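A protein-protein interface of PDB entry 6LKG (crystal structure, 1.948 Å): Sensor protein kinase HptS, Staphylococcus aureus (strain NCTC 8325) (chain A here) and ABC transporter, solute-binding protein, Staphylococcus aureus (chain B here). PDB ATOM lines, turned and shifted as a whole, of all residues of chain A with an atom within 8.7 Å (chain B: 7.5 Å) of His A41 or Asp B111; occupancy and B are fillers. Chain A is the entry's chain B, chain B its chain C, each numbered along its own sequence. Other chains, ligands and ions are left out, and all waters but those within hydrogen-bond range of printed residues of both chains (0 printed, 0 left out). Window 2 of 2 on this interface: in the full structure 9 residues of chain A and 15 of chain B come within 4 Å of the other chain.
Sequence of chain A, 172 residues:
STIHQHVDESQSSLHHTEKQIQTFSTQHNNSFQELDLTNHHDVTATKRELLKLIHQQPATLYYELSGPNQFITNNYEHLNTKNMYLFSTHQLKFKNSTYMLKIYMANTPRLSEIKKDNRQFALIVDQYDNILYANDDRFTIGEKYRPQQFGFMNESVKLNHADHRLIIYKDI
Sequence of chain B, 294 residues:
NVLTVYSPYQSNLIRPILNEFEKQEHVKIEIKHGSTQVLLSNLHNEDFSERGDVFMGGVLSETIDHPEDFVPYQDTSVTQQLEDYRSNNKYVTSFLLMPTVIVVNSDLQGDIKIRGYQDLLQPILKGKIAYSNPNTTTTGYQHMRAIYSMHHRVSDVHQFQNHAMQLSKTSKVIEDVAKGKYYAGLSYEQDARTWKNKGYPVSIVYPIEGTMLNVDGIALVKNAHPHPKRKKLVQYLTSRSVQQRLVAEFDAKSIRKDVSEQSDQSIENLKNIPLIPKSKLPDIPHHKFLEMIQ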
ATOM      1  N   LEU A  35      36.139 -19.549  21.959  1.00  0.00           N
ATOM      2  CA  LEU A  35      34.782 -19.770  21.486  1.00  0.00           C
ATOM      3  C   LEU A  35      34.808 -20.827  20.394  1.00  0.00           C
ATOM      4  O   LEU A  35      35.546 -20.695  19.411  1.00  0.00           O
ATOM      5  CB  LEU A  35      34.170 -18.472  20.956  1.00  0.00           C
ATOM      6  CG  LEU A  35      33.917 -17.366  21.983  1.00  0.00           C
ATOM      7  CD1 LEU A  35      33.522 -16.072  21.288  1.00  0.00           C
ATOM      8  CD2 LEU A  35      32.848 -17.790  22.976  1.00  0.00           C
ATOM      9  N   ASP A  36      34.002 -21.867  20.568  1.00  0.00           N
ATOM     10  CA  ASP A  36      33.875 -22.938  19.589  1.00  0.00           C
ATOM     11  C   ASP A  36      32.546 -22.733  18.876  1.00  0.00           C
ATOM     12  O   ASP A  36      31.478 -22.846  19.487  1.00  0.00           O
ATOM     13  CB  ASP A  36      33.974 -24.301  20.277  1.00  0.00           C
ATOM     14  CG  ASP A  36      33.505 -25.454  19.401  1.00  0.00           C
ATOM     15  OD1 ASP A  36      33.446 -25.315  18.162  1.00  0.00           O
ATOM     16  OD2 ASP A  36      33.224 -26.532  19.962  1.00  0.00           O
ATOM     17  N   LEU A  37      32.613 -22.449  17.579  1.00  0.00           N
ATOM     18  CA  LEU A  37      31.438 -22.082  16.802  1.00  0.00           C
ATOM     19  C   LEU A  37      30.567 -23.275  16.421  1.00  0.00           C
ATOM     20  O   LEU A  37      29.624 -23.102  15.642  1.00  0.00           O
ATOM     21  CB  LEU A  37      31.870 -21.320  15.547  1.00  0.00           C
ATOM     22  CG  LEU A  37      32.592 -19.991  15.806  1.00  0.00           C
ATOM     23  CD1 LEU A  37      32.718 -19.147  14.544  1.00  0.00           C
ATOM     24  CD2 LEU A  37      31.901 -19.202  16.910  1.00  0.00           C
ATOM     25  N   THR A  38      30.875 -24.476  16.917  1.00  0.00           N
ATOM     26  CA  THR A  38      29.947 -25.602  16.863  1.00  0.00           C
ATOM     27  C   THR A  38      29.019 -25.655  18.068  1.00  0.00           C
ATOM     28  O   THR A  38      28.083 -26.461  18.082  1.00  0.00           O
ATOM     29  CB  THR A  38      30.718 -26.918  16.772  1.00  0.00           C
ATOM     30  OG1 THR A  38      31.513 -27.078  17.950  1.00  0.00           O
ATOM     31  CG2 THR A  38      31.638 -26.892  15.583  1.00  0.00           C
ATOM     32  N   ASN A  39      29.273 -24.822  19.070  1.00  0.00           N
ATOM     33  CA  ASN A  39      28.413 -24.641  20.230  1.00  0.00           C
ATOM     34  C   ASN A  39      27.462 -23.470  19.990  1.00  0.00           C
ATOM     35  O   ASN A  39      27.893 -22.410  19.516  1.00  0.00           O
ATOM     36  CB  ASN A  39      29.303 -24.393  21.457  1.00  0.00           C
ATOM     37  CG  ASN A  39      28.525 -24.224  22.727  1.00  0.00           C
ATOM     38  OD1 ASN A  39      27.308 -24.246  22.710  1.00  0.00           O
ATOM     39  ND2 ASN A  39      29.228 -24.009  23.841  1.00  0.00           N
ATOM     40  N   HIS A  40      26.173 -23.671  20.296  1.00  0.00           N
ATOM     41  CA  HIS A  40      25.214 -22.595  20.093  1.00  0.00           C
ATOM     42  C   HIS A  40      25.446 -21.393  21.017  1.00  0.00           C
ATOM     43  O   HIS A  40      25.268 -20.248  20.575  1.00  0.00           O
ATOM     44  CB  HIS A  40      23.763 -23.147  20.128  1.00  0.00           C
ATOM     45  CG  HIS A  40      23.084 -22.974  21.456  1.00  0.00           C
ATOM     46  ND1 HIS A  40      23.528 -23.700  22.528  1.00  0.00           N
ATOM     47  CD2 HIS A  40      22.261 -22.020  21.963  1.00  0.00           C
ATOM     48  CE1 HIS A  40      22.860 -23.335  23.591  1.00  0.00           C
ATOM     49  NE2 HIS A  40      22.121 -22.288  23.288  1.00  0.00           N
ATOM     50  N   HIS A  41      26.014 -21.585  22.210  1.00  0.00           N
ATOM     51  CA  HIS A  41      26.278 -20.403  23.041  1.00  0.00           C
ATOM     52  C   HIS A  41      27.351 -19.503  22.424  1.00  0.00           C
ATOM     53  O   HIS A  41      27.171 -18.281  22.323  1.00  0.00           O
ATOM     54  CB  HIS A  41      26.728 -20.773  24.460  1.00  0.00           C
ATOM     55  CG  HIS A  41      25.905 -21.844  25.081  1.00  0.00           C
ATOM     56  ND1 HIS A  41      24.894 -21.587  25.985  1.00  0.00           N
ATOM     57  CD2 HIS A  41      26.009 -23.200  24.974  1.00  0.00           C
ATOM     58  CE1 HIS A  41      24.389 -22.754  26.368  1.00  0.00           C
ATOM     59  NE2 HIS A  41      25.045 -23.745  25.775  1.00  0.00           N
ATOM     60  N   ASP A  42      28.449 -20.102  21.954  1.00  0.00           N
ATOM     61  CA  ASP A  42      29.565 -19.338  21.408  1.00  0.00           C
ATOM     62  C   ASP A  42      29.202 -18.636  20.109  1.00  0.00           C
ATOM     63  O   ASP A  42      29.754 -17.572  19.810  1.00  0.00           O
ATOM     64  CB  ASP A  42      30.767 -20.263  21.206  1.00  0.00           C
ATOM     65  CG  ASP A  42      31.206 -20.931  22.503  1.00  0.00           C
ATOM     66  OD1 ASP A  42      30.647 -20.576  23.561  1.00  0.00           O
ATOM     67  OD2 ASP A  42      32.067 -21.841  22.462  1.00  0.00           O
ATOM     68  N   VAL A  43      28.308 -19.228  19.315  1.00  0.00           N
ATOM     69  CA  VAL A  43      27.810 -18.548  18.125  1.00  0.00           C
ATOM     70  C   VAL A  43      27.025 -17.307  18.524  1.00  0.00           C
ATOM     71  O   VAL A  43      27.200 -16.230  17.944  1.00  0.00           O
ATOM     72  CB  VAL A  43      26.961 -19.511  17.275  1.00  0.00           C
ATOM     73  CG1 VAL A  43      26.266 -18.758  16.152  1.00  0.00           C
ATOM     74  CG2 VAL A  43      27.823 -20.634  16.717  1.00  0.00           C
ATOM     75  N   THR A  44      26.153 -17.438  19.530  1.00  0.00           N
ATOM     76  CA  THR A  44      25.406 -16.283  20.019  1.00  0.00           C
ATOM     77  C   THR A  44      26.344 -15.208  20.553  1.00  0.00           C
ATOM     78  O   THR A  44      26.168 -14.018  20.260  1.00  0.00           O
ATOM     79  CB  THR A  44      24.418 -16.708  21.106  1.00  0.00           C
ATOM     80  OG1 THR A  44      23.454 -17.612  20.553  1.00  0.00           O
ATOM     81  CG2 THR A  44      23.695 -15.492  21.677  1.00  0.00           C
ATOM     82  N   ALA A  45      27.351 -15.608  21.332  1.00  0.00           N
ATOM     83  CA  ALA A  45      28.301 -14.639  21.866  1.00  0.00           C
ATOM     84  C   ALA A  45      29.065 -13.943  20.747  1.00  0.00           C
ATOM     85  O   ALA A  45      29.382 -12.752  20.848  1.00  0.00           O
ATOM     86  CB  ALA A  45      29.264 -15.326  22.833  1.00  0.00           C
ATOM     87  N   THR A  46      29.366 -14.670  19.668  1.00  0.00           N
ATOM     88  CA  THR A  46      30.071 -14.065  18.542  1.00  0.00           C
ATOM     89  C   THR A  46      29.162 -13.123  17.764  1.00  0.00           C
ATOM     90  O   THR A  46      29.587 -12.037  17.356  1.00  0.00           O
ATOM     91  CB  THR A  46      30.627 -15.154  17.623  1.00  0.00           C
ATOM     92  OG1 THR A  46      31.414 -16.074  18.389  1.00  0.00           O
ATOM     93  CG2 THR A  46      31.489 -14.538  16.528  1.00  0.00           C
ATOM     94  N   LYS A  47      27.907 -13.523  17.545  1.00  0.00           N
ATOM     95  CA  LYS A  47      26.959 -12.646  16.865  1.00  0.00           C
ATOM     96  C   LYS A  47      26.737 -11.361  17.654  1.00  0.00           C
ATOM     97  O   LYS A  47      26.613 -10.279  17.068  1.00  0.00           O
ATOM     98  CB  LYS A  47      25.634 -13.377  16.646  1.00  0.00           C
ATOM     99  CG  LYS A  47      25.669 -14.419  15.542  1.00  0.00           C
ATOM    100  CD  LYS A  47      24.334 -15.133  15.427  1.00  0.00           C
ATOM    101  CE  LYS A  47      24.313 -16.093  14.252  1.00  0.00           C
ATOM    102  NZ  LYS A  47      23.013 -16.813  14.152  1.00  0.00           N
ATOM    103  N   ARG A  48      26.688 -11.462  18.985  1.00  0.00           N
ATOM    104  CA  ARG A  48      26.505 -10.270  19.807  1.00  0.00           C
ATOM    105  C   ARG A  48      27.661  -9.293  19.631  1.00  0.00           C
ATOM    106  O   ARG A  48      27.447  -8.080  19.522  1.00  0.00           O
ATOM    107  CB  ARG A  48      26.360 -10.661  21.279  1.00  0.00           C
ATOM    108  CG  ARG A  48      25.042 -11.333  21.632  1.00  0.00           C
ATOM    109  CD  ARG A  48      25.079 -11.904  23.044  1.00  0.00           C
ATOM    110  NE  ARG A  48      23.802 -12.495  23.432  1.00  0.00           N
ATOM    111  CZ  ARG A  48      23.603 -13.177  24.556  1.00  0.00           C
ATOM    112  NH1 ARG A  48      24.599 -13.360  25.413  1.00  0.00           N
ATOM    113  NH2 ARG A  48      22.405 -13.679  24.824  1.00  0.00           N
ATOM    114  N   LEU B 108      20.463 -12.314  18.949  1.00  0.00           N
ATOM    115  CA  LEU B 108      21.029 -11.791  20.185  1.00  0.00           C
ATOM    116  C   LEU B 108      20.473 -12.451  21.440  1.00  0.00           C
ATOM    117  O   LEU B 108      21.123 -12.385  22.490  1.00  0.00           O
ATOM    118  CB  LEU B 108      20.781 -10.280  20.281  1.00  0.00           C
ATOM    119  CG  LEU B 108      21.386  -9.398  19.187  1.00  0.00           C
ATOM    120  CD1 LEU B 108      20.784  -7.999  19.240  1.00  0.00           C
ATOM    121  CD2 LEU B 108      22.897  -9.339  19.324  1.00  0.00           C
ATOM    122  N   GLN B 109      19.302 -13.089  21.354  1.00  0.00           N
ATOM    123  CA  GLN B 109      18.599 -13.526  22.558  1.00  0.00           C
ATOM    124  C   GLN B 109      19.415 -14.536  23.356  1.00  0.00           C
ATOM    125  O   GLN B 109      19.668 -14.342  24.550  1.00  0.00           O
ATOM    126  CB  GLN B 109      17.236 -14.115  22.188  1.00  0.00           C
ATOM    127  CG  GLN B 109      16.440 -14.612  23.390  1.00  0.00           C
ATOM    128  CD  GLN B 109      15.009 -14.986  23.044  1.00  0.00           C
ATOM    129  OE1 GLN B 109      14.684 -15.250  21.888  1.00  0.00           O
ATOM    130  NE2 GLN B 109      14.145 -15.011  24.053  1.00  0.00           N
ATOM    131  N   GLY B 110      19.832 -15.621  22.714  1.00  0.00           N
ATOM    132  CA  GLY B 110      20.552 -16.656  23.439  1.00  0.00           C
ATOM    133  C   GLY B 110      19.631 -17.327  24.441  1.00  0.00           C
ATOM    134  O   GLY B 110      18.515 -17.739  24.107  1.00  0.00           O
ATOM    135  N   ASP B 111      20.089 -17.422  25.687  1.00  0.00           N
ATOM    136  CA  ASP B 111      19.304 -18.024  26.758  1.00  0.00           C
ATOM    137  C   ASP B 111      18.473 -17.014  27.534  1.00  0.00           C
ATOM    138  O   ASP B 111      17.823 -17.397  28.512  1.00  0.00           O
ATOM    139  CB  ASP B 111      20.209 -18.787  27.731  1.00  0.00           C
ATOM    140  CG  ASP B 111      20.681 -20.111  27.169  1.00  0.00           C
ATOM    141  OD1 ASP B 111      20.038 -20.620  26.227  1.00  0.00           O
ATOM    142  OD2 ASP B 111      21.683 -20.652  27.683  1.00  0.00           O
ATOM    143  N   ILE B 112      18.486 -15.741  27.143  1.00  0.00           N
ATOM    144  CA  ILE B 112      17.699 -14.743  27.858  1.00  0.00           C
ATOM    145  C   ILE B 112      16.222 -15.033  27.621  1.00  0.00           C
ATOM    146  O   ILE B 112      15.742 -14.998  26.482  1.00  0.00           O
ATOM    147  CB  ILE B 112      18.067 -13.323  27.413  1.00  0.00           C
ATOM    148  CG1 ILE B 112      19.565 -13.073  27.606  1.00  0.00           C
ATOM    149  CG2 ILE B 112      17.248 -12.296  28.180  1.00  0.00           C
ATOM    150  CD1 ILE B 112      20.036 -11.746  27.049  1.00  0.00           C
ATOM    151  N   LYS B 113      15.499 -15.325  28.697  1.00  0.00           N
ATOM    152  CA  LYS B 113      14.076 -15.610  28.597  1.00  0.00           C
ATOM    153  C   LYS B 113      13.303 -14.311  28.419  1.00  0.00           C
ATOM    154  O   LYS B 113      13.447 -13.378  29.214  1.00  0.00           O
ATOM    155  CB  LYS B 113      13.599 -16.351  29.845  1.00  0.00           C
ATOM    156  CG  LYS B 113      12.147 -16.795  29.805  1.00  0.00           C
ATOM    157  CD  LYS B 113      11.765 -17.522  31.088  1.00  0.00           C
ATOM    158  CE  LYS B 113      11.175 -16.566  32.116  1.00  0.00           C
ATOM    159  NZ  LYS B 113       9.802 -16.119  31.744  1.00  0.00           N
ATOM    160  N   ILE B 114      12.494 -14.246  27.362  1.00  0.00           N
ATOM    161  CA  ILE B 114      11.658 -13.079  27.101  1.00  0.00           C
ATOM    162  C   ILE B 114      10.264 -13.541  26.707  1.00  0.00           C
ATOM    163  O   ILE B 114      10.007 -13.851  25.537  1.00  0.00           O
ATOM    164  CB  ILE B 114      12.263 -12.176  26.009  1.00  0.00           C
ATOM    165  CG1 ILE B 114      13.671 -11.720  26.396  1.00  0.00           C
ATOM    166  CG2 ILE B 114      11.368 -10.965  25.778  1.00  0.00           C
ATOM    167  CD1 ILE B 114      14.344 -10.853  25.355  1.00  0.00           C
ATOM    168  N   GLN B 122      14.988  -7.788  33.211  1.00  0.00           N
ATOM    169  CA  GLN B 122      16.218  -8.462  33.605  1.00  0.00           C
ATOM    170  C   GLN B 122      17.393  -7.498  33.472  1.00  0.00           C
ATOM    171  O   GLN B 122      17.488  -6.782  32.465  1.00  0.00           O
ATOM    172  CB  GLN B 122      16.461  -9.706  32.751  1.00  0.00           C
ATOM    173  CG  GLN B 122      15.532 -10.869  33.058  1.00  0.00           C
ATOM    174  CD  GLN B 122      15.674 -12.004  32.064  1.00  0.00           C
ATOM    175  OE1 GLN B 122      16.552 -12.858  32.198  1.00  0.00           O
ATOM    176  NE2 GLN B 122      14.813 -12.016  31.051  1.00  0.00           N
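NE of Arg A48 sits at hydrogen-bond distance from O of Leu B108.
The guanidinium group (NH2) of Arg A48 is in hydrogen-bond range of the backbone carbonyl oxygen (O) of Gln B109, at 2.8 Å.
OD1 of Asn A39 lies close to N of His A41 (3.0 Å).
O of His A40 lies within hydrogen-bond range of OG1 of Thr A44 (3.2 Å).
The side-chain amide nitrogen (NE2) of Gln B109 lies within hydrogen-bond range of the backbone carbonyl oxygen (O) of Ile B112, at 2.9 Å.
Among the printed residues, pairs that only touch across the chains: His A41 with Asp B111 (3.7 Å), Arg A48 with Gly B110 (3.8 Å), Arg A48 with Ile B112 (3.8 Å), Thr A44 with Gly B110 (3.8 Å) and His A40 with Asp B111 (3.97 Å).
Of the printed residues of chain B, His A40 touches Asp B111.
Printed residues of chain B within 4 Å of Thr A44: Gly B110.
Lys A47 touches none of the printed residues of chain B.
Of the printed residues of chain B, Arg A48 touches Leu B108, Gln B109, Gly B110 and Ile B112.
Printed residues of chain A within 4 Å of Gln B109: Arg A48 (2.8 Å).
Gly B110 touches just these residues of chain A: Thr A44 (3.8 Å) and Arg A48 (3.8 Å).
Of chain A, only His A40 and His A41 come within 4 Å of Asp B111.
Printed residues of chain A within 4 Å of Ile B112: Arg A48.
Lys B113 touches none of the printed residues of chain A.
The nearest residue of chain B that does not touch His A41 is Gly B110 (6.9 Å).
The nearest residue of chain A that does not touch Asp B111 is Arg A48 (4.5 Å).
Of the 8 printed residues of chain B, 5 touch a printed residue of chain A.
Printed residues of chain A that touch a printed residue of chain B: His A40, His A41, Thr A44 and Arg A48.
Among the printed residues, 7 pairs touch across the chains.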
